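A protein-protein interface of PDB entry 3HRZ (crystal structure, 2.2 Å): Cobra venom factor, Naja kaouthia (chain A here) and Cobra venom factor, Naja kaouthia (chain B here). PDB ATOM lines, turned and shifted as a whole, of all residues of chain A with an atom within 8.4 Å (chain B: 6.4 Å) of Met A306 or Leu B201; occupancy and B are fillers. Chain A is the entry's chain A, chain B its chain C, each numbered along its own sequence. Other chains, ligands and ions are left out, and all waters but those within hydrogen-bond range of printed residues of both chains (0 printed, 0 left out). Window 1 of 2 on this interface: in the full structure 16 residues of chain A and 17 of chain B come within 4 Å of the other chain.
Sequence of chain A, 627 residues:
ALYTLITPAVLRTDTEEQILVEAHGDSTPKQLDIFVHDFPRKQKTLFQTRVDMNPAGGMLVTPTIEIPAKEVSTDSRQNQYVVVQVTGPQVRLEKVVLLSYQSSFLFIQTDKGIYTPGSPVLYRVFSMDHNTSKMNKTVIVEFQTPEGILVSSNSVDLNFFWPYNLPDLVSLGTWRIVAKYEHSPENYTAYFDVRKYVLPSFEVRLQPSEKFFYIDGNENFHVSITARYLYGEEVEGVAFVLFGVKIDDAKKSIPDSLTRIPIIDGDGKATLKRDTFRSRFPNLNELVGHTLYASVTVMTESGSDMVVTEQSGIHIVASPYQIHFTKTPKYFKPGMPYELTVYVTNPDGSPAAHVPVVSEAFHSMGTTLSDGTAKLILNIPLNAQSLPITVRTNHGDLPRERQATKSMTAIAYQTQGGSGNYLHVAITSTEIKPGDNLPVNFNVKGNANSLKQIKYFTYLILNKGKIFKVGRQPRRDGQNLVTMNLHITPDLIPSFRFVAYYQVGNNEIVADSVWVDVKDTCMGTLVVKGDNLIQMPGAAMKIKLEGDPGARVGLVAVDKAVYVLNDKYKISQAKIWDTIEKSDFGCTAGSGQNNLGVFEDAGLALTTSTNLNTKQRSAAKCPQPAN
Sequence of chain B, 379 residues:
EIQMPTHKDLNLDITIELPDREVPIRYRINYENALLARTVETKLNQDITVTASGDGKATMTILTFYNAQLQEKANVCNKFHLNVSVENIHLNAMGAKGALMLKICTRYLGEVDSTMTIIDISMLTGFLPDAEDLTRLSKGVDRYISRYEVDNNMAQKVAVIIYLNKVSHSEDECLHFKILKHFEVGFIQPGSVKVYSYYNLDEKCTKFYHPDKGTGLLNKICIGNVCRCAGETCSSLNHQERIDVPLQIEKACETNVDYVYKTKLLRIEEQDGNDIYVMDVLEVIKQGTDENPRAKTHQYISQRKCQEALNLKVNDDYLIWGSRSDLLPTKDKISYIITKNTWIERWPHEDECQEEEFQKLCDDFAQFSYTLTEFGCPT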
ATOM      1  N   VAL A 198      -0.899 -19.269   9.959  1.00  0.00           N
ATOM      2  CA  VAL A 198      -2.314 -18.997   9.791  1.00  0.00           C
ATOM      3  C   VAL A 198      -2.530 -18.715   8.310  1.00  0.00           C
ATOM      4  O   VAL A 198      -1.619 -18.251   7.628  1.00  0.00           O
ATOM      5  CB  VAL A 198      -2.760 -17.786  10.624  1.00  0.00           C
ATOM      6  CG1 VAL A 198      -2.293 -17.935  12.082  1.00  0.00           C
ATOM      7  CG2 VAL A 198      -2.212 -16.531  10.031  1.00  0.00           C
ATOM      8  N   LEU A 199      -3.722 -19.006   7.806  1.00  0.00           N
ATOM      9  CA  LEU A 199      -3.992 -18.805   6.391  1.00  0.00           C
ATOM     10  C   LEU A 199      -4.046 -17.324   6.097  1.00  0.00           C
ATOM     11  O   LEU A 199      -4.738 -16.589   6.789  1.00  0.00           O
ATOM     12  CB  LEU A 199      -5.331 -19.429   5.992  1.00  0.00           C
ATOM     13  CG  LEU A 199      -5.537 -20.926   6.197  1.00  0.00           C
ATOM     14  CD1 LEU A 199      -6.953 -21.308   5.767  1.00  0.00           C
ATOM     15  CD2 LEU A 199      -4.489 -21.753   5.461  1.00  0.00           C
ATOM     16  N   PRO A 200      -3.330 -16.879   5.052  1.00  0.00           N
ATOM     17  CA  PRO A 200      -3.457 -15.477   4.644  1.00  0.00           C
ATOM     18  C   PRO A 200      -4.830 -15.266   4.029  1.00  0.00           C
ATOM     19  O   PRO A 200      -5.508 -16.229   3.674  1.00  0.00           O
ATOM     20  CB  PRO A 200      -2.376 -15.311   3.570  1.00  0.00           C
ATOM     21  CG  PRO A 200      -1.721 -16.640   3.403  1.00  0.00           C
ATOM     22  CD  PRO A 200      -2.541 -17.671   4.100  1.00  0.00           C
ATOM     23  N   SER A 201      -5.238 -14.013   3.910  1.00  0.00           N
ATOM     24  CA  SER A 201      -6.517 -13.647   3.317  1.00  0.00           C
ATOM     25  C   SER A 201      -6.383 -13.377   1.809  1.00  0.00           C
ATOM     26  O   SER A 201      -7.397 -13.166   1.118  1.00  0.00           O
ATOM     27  CB  SER A 201      -7.056 -12.393   4.000  1.00  0.00           C
ATOM     28  OG  SER A 201      -6.073 -11.366   3.994  1.00  0.00           O
ATOM     29  N   PHE A 202      -5.155 -13.386   1.294  1.00  0.00           N
ATOM     30  CA  PHE A 202      -4.981 -13.110  -0.131  1.00  0.00           C
ATOM     31  C   PHE A 202      -3.844 -13.893  -0.757  1.00  0.00           C
ATOM     32  O   PHE A 202      -2.974 -14.422  -0.072  1.00  0.00           O
ATOM     33  CB  PHE A 202      -4.793 -11.611  -0.396  1.00  0.00           C
ATOM     34  CG  PHE A 202      -3.500 -11.060   0.119  1.00  0.00           C
ATOM     35  CD1 PHE A 202      -2.422 -10.865  -0.738  1.00  0.00           C
ATOM     36  CD2 PHE A 202      -3.352 -10.743   1.463  1.00  0.00           C
ATOM     37  CE1 PHE A 202      -1.214 -10.336  -0.263  1.00  0.00           C
ATOM     38  CE2 PHE A 202      -2.155 -10.230   1.947  1.00  0.00           C
ATOM     39  CZ  PHE A 202      -1.078 -10.022   1.076  1.00  0.00           C
ATOM     40  N   VAL A 204      -0.768 -14.118  -3.884  1.00  0.00           N
ATOM     41  CA  VAL A 204       0.138 -13.318  -4.689  1.00  0.00           C
ATOM     42  C   VAL A 204       0.594 -14.125  -5.905  1.00  0.00           C
ATOM     43  O   VAL A 204       1.156 -15.217  -5.771  1.00  0.00           O
ATOM     44  CB  VAL A 204       1.340 -12.861  -3.865  1.00  0.00           C
ATOM     45  CG1 VAL A 204       2.437 -12.317  -4.767  1.00  0.00           C
ATOM     46  CG2 VAL A 204       0.904 -11.807  -2.834  1.00  0.00           C
ATOM     47  N   VAL A 238       1.573  -2.681  -0.306  1.00  0.00           N
ATOM     48  CA  VAL A 238       2.972  -2.408  -0.613  1.00  0.00           C
ATOM     49  C   VAL A 238       3.697  -3.748  -0.772  1.00  0.00           C
ATOM     50  O   VAL A 238       3.316  -4.736  -0.141  1.00  0.00           O
ATOM     51  CB  VAL A 238       3.618  -1.555   0.519  1.00  0.00           C
ATOM     52  CG1 VAL A 238       5.109  -1.458   0.348  1.00  0.00           C
ATOM     53  CG2 VAL A 238       3.000  -0.138   0.558  1.00  0.00           C
ATOM     54  N   PHE A 240       7.756  -5.549  -1.045  1.00  0.00           N
ATOM     55  CA  PHE A 240       9.201  -5.428  -0.904  1.00  0.00           C
ATOM     56  C   PHE A 240       9.828  -6.586  -1.690  1.00  0.00           C
ATOM     57  O   PHE A 240       9.596  -7.771  -1.389  1.00  0.00           O
ATOM     58  CB  PHE A 240       9.611  -5.501   0.567  1.00  0.00           C
ATOM     59  CG  PHE A 240       9.125  -4.345   1.394  1.00  0.00           C
ATOM     60  CD1 PHE A 240       9.880  -3.188   1.509  1.00  0.00           C
ATOM     61  CD2 PHE A 240       7.906  -4.408   2.049  1.00  0.00           C
ATOM     62  CE1 PHE A 240       9.427  -2.107   2.277  1.00  0.00           C
ATOM     63  CE2 PHE A 240       7.448  -3.342   2.818  1.00  0.00           C
ATOM     64  CZ  PHE A 240       8.212  -2.188   2.930  1.00  0.00           C
ATOM     65  N   SER A 295      12.412 -12.609  -4.246  1.00  0.00           N
ATOM     66  CA  SER A 295      11.596 -12.730  -3.049  1.00  0.00           C
ATOM     67  C   SER A 295      10.605 -11.557  -2.981  1.00  0.00           C
ATOM     68  O   SER A 295      11.007 -10.400  -2.984  1.00  0.00           O
ATOM     69  CB  SER A 295      12.490 -12.751  -1.819  1.00  0.00           C
ATOM     70  OG  SER A 295      11.697 -12.743  -0.651  1.00  0.00           O
ATOM     71  N   VAL A 296       9.314 -11.870  -2.962  1.00  0.00           N
ATOM     72  CA  VAL A 296       8.253 -10.871  -2.962  1.00  0.00           C
ATOM     73  C   VAL A 296       7.449 -10.979  -1.654  1.00  0.00           C
ATOM     74  O   VAL A 296       6.888 -12.033  -1.345  1.00  0.00           O
ATOM     75  CB  VAL A 296       7.320 -11.040  -4.164  1.00  0.00           C
ATOM     76  CG1 VAL A 296       6.221 -10.004  -4.134  1.00  0.00           C
ATOM     77  CG2 VAL A 296       8.103 -10.933  -5.485  1.00  0.00           C
ATOM     78  N   THR A 297       7.442  -9.894  -0.875  1.00  0.00           N
ATOM     79  CA  THR A 297       6.700  -9.827   0.379  1.00  0.00           C
ATOM     80  C   THR A 297       5.674  -8.719   0.237  1.00  0.00           C
ATOM     81  O   THR A 297       6.036  -7.547   0.084  1.00  0.00           O
ATOM     82  CB  THR A 297       7.620  -9.516   1.562  1.00  0.00           C
ATOM     83  OG1 THR A 297       8.605 -10.550   1.681  1.00  0.00           O
ATOM     84  CG2 THR A 297       6.812  -9.406   2.914  1.00  0.00           C
ATOM     85  N   VAL A 298       4.393  -9.085   0.247  1.00  0.00           N
ATOM     86  CA  VAL A 298       3.333  -8.097   0.075  1.00  0.00           C
ATOM     87  C   VAL A 298       2.603  -7.872   1.402  1.00  0.00           C
ATOM     88  O   VAL A 298       2.243  -8.840   2.076  1.00  0.00           O
ATOM     89  CB  VAL A 298       2.324  -8.549  -0.992  1.00  0.00           C
ATOM     90  CG1 VAL A 298       1.134  -7.577  -1.078  1.00  0.00           C
ATOM     91  CG2 VAL A 298       3.021  -8.684  -2.362  1.00  0.00           C
ATOM     92  N   MET A 299       2.395  -6.604   1.770  1.00  0.00           N
ATOM     93  CA  MET A 299       1.574  -6.247   2.933  1.00  0.00           C
ATOM     94  C   MET A 299       0.328  -5.492   2.498  1.00  0.00           C
ATOM     95  O   MET A 299       0.403  -4.629   1.620  1.00  0.00           O
ATOM     96  CB  MET A 299       2.364  -5.356   3.887  1.00  0.00           C
ATOM     97  CG  MET A 299       3.651  -5.987   4.328  1.00  0.00           C
ATOM     98  SD  MET A 299       4.764  -4.799   5.049  1.00  0.00           S
ATOM     99  CE  MET A 299       6.234  -5.803   5.244  1.00  0.00           C
ATOM    100  N   THR A 300      -0.814  -5.780   3.115  1.00  0.00           N
ATOM    101  CA  THR A 300      -2.005  -4.998   2.798  1.00  0.00           C
ATOM    102  C   THR A 300      -1.794  -3.577   3.319  1.00  0.00           C
ATOM    103  O   THR A 300      -0.956  -3.365   4.196  1.00  0.00           O
ATOM    104  CB  THR A 300      -3.255  -5.600   3.418  1.00  0.00           C
ATOM    105  OG1 THR A 300      -3.102  -5.627   4.838  1.00  0.00           O
ATOM    106  CG2 THR A 300      -3.453  -7.043   2.926  1.00  0.00           C
ATOM    107  N   GLY A 303      -1.917  -3.033   7.009  1.00  0.00           N
ATOM    108  CA  GLY A 303      -0.967  -3.790   7.823  1.00  0.00           C
ATOM    109  C   GLY A 303      -1.577  -4.999   8.539  1.00  0.00           C
ATOM    110  O   GLY A 303      -0.960  -5.600   9.419  1.00  0.00           O
ATOM    111  N   SER A 304      -2.798  -5.361   8.169  1.00  0.00           N
ATOM    112  CA  SER A 304      -3.482  -6.483   8.799  1.00  0.00           C
ATOM    113  C   SER A 304      -2.968  -7.845   8.314  1.00  0.00           C
ATOM    114  O   SER A 304      -3.211  -8.866   8.951  1.00  0.00           O
ATOM    115  CB  SER A 304      -4.986  -6.395   8.523  1.00  0.00           C
ATOM    116  OG  SER A 304      -5.233  -6.416   7.123  1.00  0.00           O
ATOM    117  N   ASP A 305      -2.287  -7.872   7.173  1.00  0.00           N
ATOM    118  CA  ASP A 305      -1.858  -9.144   6.609  1.00  0.00           C
ATOM    119  C   ASP A 305      -0.659  -9.024   5.666  1.00  0.00           C
ATOM    120  O   ASP A 305      -0.442  -7.992   5.031  1.00  0.00           O
ATOM    121  CB  ASP A 305      -3.037  -9.803   5.903  1.00  0.00           C
ATOM    122  CG  ASP A 305      -2.908 -11.329   5.821  1.00  0.00           C
ATOM    123  OD1 ASP A 305      -1.971 -11.922   6.417  1.00  0.00           O
ATOM    124  OD2 ASP A 305      -3.770 -11.935   5.145  1.00  0.00           O
ATOM    125  N   MET A 306       0.098 -10.109   5.573  1.00  0.00           N
ATOM    126  CA  MET A 306       1.321 -10.165   4.799  1.00  0.00           C
ATOM    127  C   MET A 306       1.451 -11.539   4.122  1.00  0.00           C
ATOM    128  O   MET A 306       1.097 -12.569   4.709  1.00  0.00           O
ATOM    129  CB  MET A 306       2.506  -9.950   5.748  1.00  0.00           C
ATOM    130  CG  MET A 306       3.854  -9.842   5.063  1.00  0.00           C
ATOM    131  SD  MET A 306       5.172  -9.459   6.240  1.00  0.00           S
ATOM    132  CE  MET A 306       4.948 -10.759   7.440  1.00  0.00           C
ATOM    133  N   VAL A 307       1.972 -11.554   2.901  1.00  0.00           N
ATOM    134  CA  VAL A 307       2.258 -12.799   2.210  1.00  0.00           C
ATOM    135  C   VAL A 307       3.679 -12.755   1.634  1.00  0.00           C
ATOM    136  O   VAL A 307       4.073 -11.762   1.011  1.00  0.00           O
ATOM    137  CB  VAL A 307       1.269 -13.045   1.073  1.00  0.00           C
ATOM    138  CG1 VAL A 307       1.818 -14.124   0.073  1.00  0.00           C
ATOM    139  CG2 VAL A 307      -0.067 -13.451   1.639  1.00  0.00           C
ATOM    140  N   VAL A 308       4.450 -13.817   1.868  1.00  0.00           N
ATOM    141  CA  VAL A 308       5.797 -13.920   1.324  1.00  0.00           C
ATOM    142  C   VAL A 308       5.846 -15.044   0.295  1.00  0.00           C
ATOM    143  O   VAL A 308       5.578 -16.203   0.628  1.00  0.00           O
ATOM    144  CB  VAL A 308       6.831 -14.288   2.406  1.00  0.00           C
ATOM    145  CG1 VAL A 308       8.226 -14.360   1.783  1.00  0.00           C
ATOM    146  CG2 VAL A 308       6.792 -13.309   3.571  1.00  0.00           C
ATOM    147  N   THR A 309       6.172 -14.714  -0.948  1.00  0.00           N
ATOM    148  CA  THR A 309       6.403 -15.749  -1.942  1.00  0.00           C
ATOM    149  C   THR A 309       7.633 -15.410  -2.751  1.00  0.00           C
ATOM    150  O   THR A 309       8.264 -14.382  -2.537  1.00  0.00           O
ATOM    151  CB  THR A 309       5.211 -15.950  -2.887  1.00  0.00           C
ATOM    152  OG1 THR A 309       4.687 -14.676  -3.266  1.00  0.00           O
ATOM    153  CG2 THR A 309       4.113 -16.766  -2.198  1.00  0.00           C
ATOM    154  N   VAL A 564      -1.379 -20.866  -1.152  1.00  0.00           N
ATOM    155  CA  VAL A 564      -0.595 -19.643  -1.017  1.00  0.00           C
ATOM    156  C   VAL A 564       0.639 -19.902  -0.149  1.00  0.00           C
ATOM    157  O   VAL A 564       1.716 -19.363  -0.400  1.00  0.00           O
ATOM    158  CB  VAL A 564      -1.452 -18.470  -0.407  1.00  0.00           C
ATOM    159  CG1 VAL A 564      -0.580 -17.306   0.045  1.00  0.00           C
ATOM    160  CG2 VAL A 564      -2.512 -17.998  -1.394  1.00  0.00           C
ATOM    161  N   LEU A 565       0.475 -20.737   0.871  1.00  0.00           N
ATOM    162  CA  LEU A 565       1.575 -21.075   1.768  1.00  0.00           C
ATOM    163  C   LEU A 565       2.443 -22.204   1.213  1.00  0.00           C
ATOM    164  O   LEU A 565       3.675 -22.186   1.380  1.00  0.00           O
ATOM    165  CB  LEU A 565       1.032 -21.453   3.151  1.00  0.00           C
ATOM    166  CG  LEU A 565       0.272 -20.332   3.878  1.00  0.00           C
ATOM    167  CD1 LEU A 565      -0.481 -20.875   5.082  1.00  0.00           C
ATOM    168  CD2 LEU A 565       1.202 -19.185   4.289  1.00  0.00           C
ATOM    169  N   ILE B 118       9.455   0.016   9.085  1.00  0.00           N
ATOM    170  CA  ILE B 118       8.022   0.277   9.069  1.00  0.00           C
ATOM    171  C   ILE B 118       7.493   0.704  10.453  1.00  0.00           C
ATOM    172  O   ILE B 118       7.762   0.039  11.465  1.00  0.00           O
ATOM    173  CB  ILE B 118       7.273  -0.955   8.527  1.00  0.00           C
ATOM    174  CG1 ILE B 118       7.793  -1.262   7.106  1.00  0.00           C
ATOM    175  CG2 ILE B 118       5.773  -0.723   8.589  1.00  0.00           C
ATOM    176  CD1 ILE B 118       7.411  -2.603   6.540  1.00  0.00           C
ATOM    177  N   TYR B 196       8.974  -2.429  12.921  1.00  0.00           N
ATOM    178  CA  TYR B 196       9.739  -3.566  12.437  1.00  0.00           C
ATOM    179  C   TYR B 196      10.374  -3.166  11.110  1.00  0.00           C
ATOM    180  O   TYR B 196      10.185  -2.036  10.651  1.00  0.00           O
ATOM    181  CB  TYR B 196       8.841  -4.797  12.290  1.00  0.00           C
ATOM    182  CG  TYR B 196       7.532  -4.500  11.619  1.00  0.00           C
ATOM    183  CD1 TYR B 196       7.405  -4.585  10.237  1.00  0.00           C
ATOM    184  CD2 TYR B 196       6.414  -4.119  12.366  1.00  0.00           C
ATOM    185  CE1 TYR B 196       6.200  -4.304   9.605  1.00  0.00           C
ATOM    186  CE2 TYR B 196       5.204  -3.836  11.749  1.00  0.00           C
ATOM    187  CZ  TYR B 196       5.111  -3.922  10.364  1.00  0.00           C
ATOM    188  OH  TYR B 196       3.921  -3.641   9.738  1.00  0.00           O
ATOM    189  N   SER B 197      11.159  -4.057  10.509  1.00  0.00           N
ATOM    190  CA  SER B 197      11.816  -3.729   9.244  1.00  0.00           C
ATOM    191  C   SER B 197      11.952  -4.968   8.381  1.00  0.00           C
ATOM    192  O   SER B 197      11.740  -6.093   8.862  1.00  0.00           O
ATOM    193  CB  SER B 197      13.194  -3.107   9.484  1.00  0.00           C
ATOM    194  OG  SER B 197      14.136  -4.079   9.921  1.00  0.00           O
ATOM    195  N   TYR B 198      12.349  -4.760   7.126  1.00  0.00           N
ATOM    196  CA  TYR B 198      12.370  -5.818   6.135  1.00  0.00           C
ATOM    197  C   TYR B 198      13.164  -7.043   6.577  1.00  0.00           C
ATOM    198  O   TYR B 198      12.675  -8.165   6.486  1.00  0.00           O
ATOM    199  CB  TYR B 198      12.883  -5.313   4.781  1.00  0.00           C
ATOM    200  CG  TYR B 198      12.960  -6.438   3.782  1.00  0.00           C
ATOM    201  CD1 TYR B 198      11.830  -6.869   3.102  1.00  0.00           C
ATOM    202  CD2 TYR B 198      14.142  -7.111   3.571  1.00  0.00           C
ATOM    203  CE1 TYR B 198      11.890  -7.918   2.216  1.00  0.00           C
ATOM    204  CE2 TYR B 198      14.214  -8.159   2.690  1.00  0.00           C
ATOM    205  CZ  TYR B 198      13.091  -8.562   2.018  1.00  0.00           C
ATOM    206  OH  TYR B 198      13.195  -9.617   1.150  1.00  0.00           O
ATOM    207  N   TYR B 199      14.387  -6.828   7.055  1.00  0.00           N
ATOM    208  CA  TYR B 199      15.222  -7.928   7.492  1.00  0.00           C
ATOM    209  C   TYR B 199      14.954  -8.379   8.931  1.00  0.00           C
ATOM    210  O   TYR B 199      15.633  -9.281   9.423  1.00  0.00           O
ATOM    211  CB  TYR B 199      16.702  -7.586   7.322  1.00  0.00           C
ATOM    212  CG  TYR B 199      17.145  -7.466   5.881  1.00  0.00           C
ATOM    213  CD1 TYR B 199      17.330  -8.602   5.091  1.00  0.00           C
ATOM    214  CD2 TYR B 199      17.377  -6.220   5.310  1.00  0.00           C
ATOM    215  CE1 TYR B 199      17.751  -8.498   3.751  1.00  0.00           C
ATOM    216  CE2 TYR B 199      17.790  -6.100   3.995  1.00  0.00           C
ATOM    217  CZ  TYR B 199      17.976  -7.244   3.212  1.00  0.00           C
ATOM    218  OH  TYR B 199      18.392  -7.112   1.909  1.00  0.00           O
ATOM    219  N   ASN B 200      13.982  -7.745   9.592  1.00  0.00           N
ATOM    220  CA  ASN B 200      13.578  -8.125  10.948  1.00  0.00           C
ATOM    221  C   ASN B 200      12.061  -8.116  11.084  1.00  0.00           C
ATOM    222  O   ASN B 200      11.514  -7.414  11.951  1.00  0.00           O
ATOM    223  CB  ASN B 200      14.133  -7.142  11.987  1.00  0.00           C
ATOM    224  CG  ASN B 200      15.631  -7.017  11.943  1.00  0.00           C
ATOM    225  OD1 ASN B 200      16.161  -5.930  11.706  1.00  0.00           O
ATOM    226  ND2 ASN B 200      16.332  -8.123  12.189  1.00  0.00           N
ATOM    227  N   LEU B 201      11.378  -8.844  10.210  1.00  0.00           N
ATOM    228  CA  LEU B 201       9.919  -8.907  10.261  1.00  0.00           C
ATOM    229  C   LEU B 201       9.510  -9.841  11.389  1.00  0.00           C
ATOM    230  O   LEU B 201       8.338 -10.130  11.566  1.00  0.00           O
ATOM    231  CB  LEU B 201       9.346  -9.418   8.939  1.00  0.00           C
ATOM    232  CG  LEU B 201       9.551  -8.563   7.691  1.00  0.00           C
ATOM    233  CD1 LEU B 201       9.137  -9.352   6.455  1.00  0.00           C
ATOM    234  CD2 LEU B 201       8.780  -7.268   7.803  1.00  0.00           C
ATOM    235  N   ASP B 202      10.512 -10.332  12.110  1.00  0.00           N
ATOM    236  CA  ASP B 202      10.349 -11.159  13.295  1.00  0.00           C
ATOM    237  C   ASP B 202       9.946 -10.302  14.477  1.00  0.00           C
ATOM    238  O   ASP B 202       9.201 -10.732  15.350  1.00  0.00           O
ATOM    239  CB  ASP B 202      11.706 -11.759  13.652  1.00  0.00           C
ATOM    240  CG  ASP B 202      11.866 -13.153  13.162  1.00  0.00           C
ATOM    241  OD1 ASP B 202      10.885 -13.694  12.612  1.00  0.00           O
ATOM    242  OD2 ASP B 202      12.971 -13.710  13.344  1.00  0.00           O
ATOM    243  N   GLU B 203      10.504  -9.096  14.497  1.00  0.00           N
ATOM    244  CA  GLU B 203      10.455  -8.184  15.634  1.00  0.00           C
ATOM    245  C   GLU B 203       9.058  -7.943  16.163  1.00  0.00           C
ATOM    246  O   GLU B 203       8.198  -7.439  15.443  1.00  0.00           O
ATOM    247  CB  GLU B 203      11.063  -6.830  15.236  1.00  0.00           C
ATOM    248  CG  GLU B 203      10.966  -5.736  16.300  1.00  0.00           C
ATOM    249  CD  GLU B 203      12.032  -5.879  17.387  1.00  0.00           C
ATOM    250  OE1 GLU B 203      12.925  -6.748  17.247  1.00  0.00           O
ATOM    251  OE2 GLU B 203      11.984  -5.115  18.372  1.00  0.00           O
ATOM    252  N   LYS B 204       8.846  -8.287  17.434  1.00  0.00           N
ATOM    253  CA  LYS B 204       7.659  -7.866  18.154  1.00  0.00           C
ATOM    254  C   LYS B 204       8.036  -6.630  18.972  1.00  0.00           C
ATOM    255  O   LYS B 204       8.526  -6.747  20.097  1.00  0.00           O
ATOM    256  CB  LYS B 204       7.184  -8.959  19.115  1.00  0.00           C
ATOM    257  CG  LYS B 204       7.123 -10.359  18.537  1.00  0.00           C
ATOM    258  CD  LYS B 204       5.705 -10.742  18.146  1.00  0.00           C
ATOM    259  CE  LYS B 204       5.630 -12.206  17.722  1.00  0.00           C
ATOM    260  NZ  LYS B 204       6.167 -13.131  18.763  1.00  0.00           N
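Among the printed residues, merely in contact across the chains: Phe A240 with Tyr B198 (3.6 Å), Met A299 with Ile B118 (3.6 Å), Phe A240 with Ile B118 (3.7 Å), Met A299 with Leu B201 (3.9 Å), Ser A295 with Tyr B198 (3.9 Å) and Met A306 with Leu B201 (3.97 Å).
O of Val A238 lies within hydrogen-bond range of N of Met A299 (2.8 Å). The backbone NH (N) of Phe A240 lies within hydrogen-bond range of the backbone carbonyl oxygen (O) of Thr A297. The backbone NH of Ile B118 is in hydrogen-bond range of the backbone carbonyl oxygen of Tyr B196, 2.7 Å away.
Printed residues of chain B within 4 Å of Phe A240: Ile B118 (3.7 Å) and Tyr B198 (3.6 Å). Of the printed residues of chain B, Ser A295 touches Tyr B198. Of chain B, only Leu B201 (3.97 Å) comes within 4 Å of Met A306. Leu B201 touches two residues of chain A. The nearest residue of chain B that does not touch Met A306 is Tyr B196 (6.2 Å).
Of the 10 printed residues of chain B, 3 touch a printed residue of chain A. Of the 23 printed residues of chain A, 4 touch a printed residue of chain B. Hydrophobic or aromatic side chains of chain A within 4 Å of the printed part of chain B: Phe A240, Met A299 and Met A306. Among the printed residues, 6 pairs touch across the chains. Among the printed residues, no Asp or Glu carboxylate lies within 4 Å of a Lys or Arg side-chain nitrogen of the other chain.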
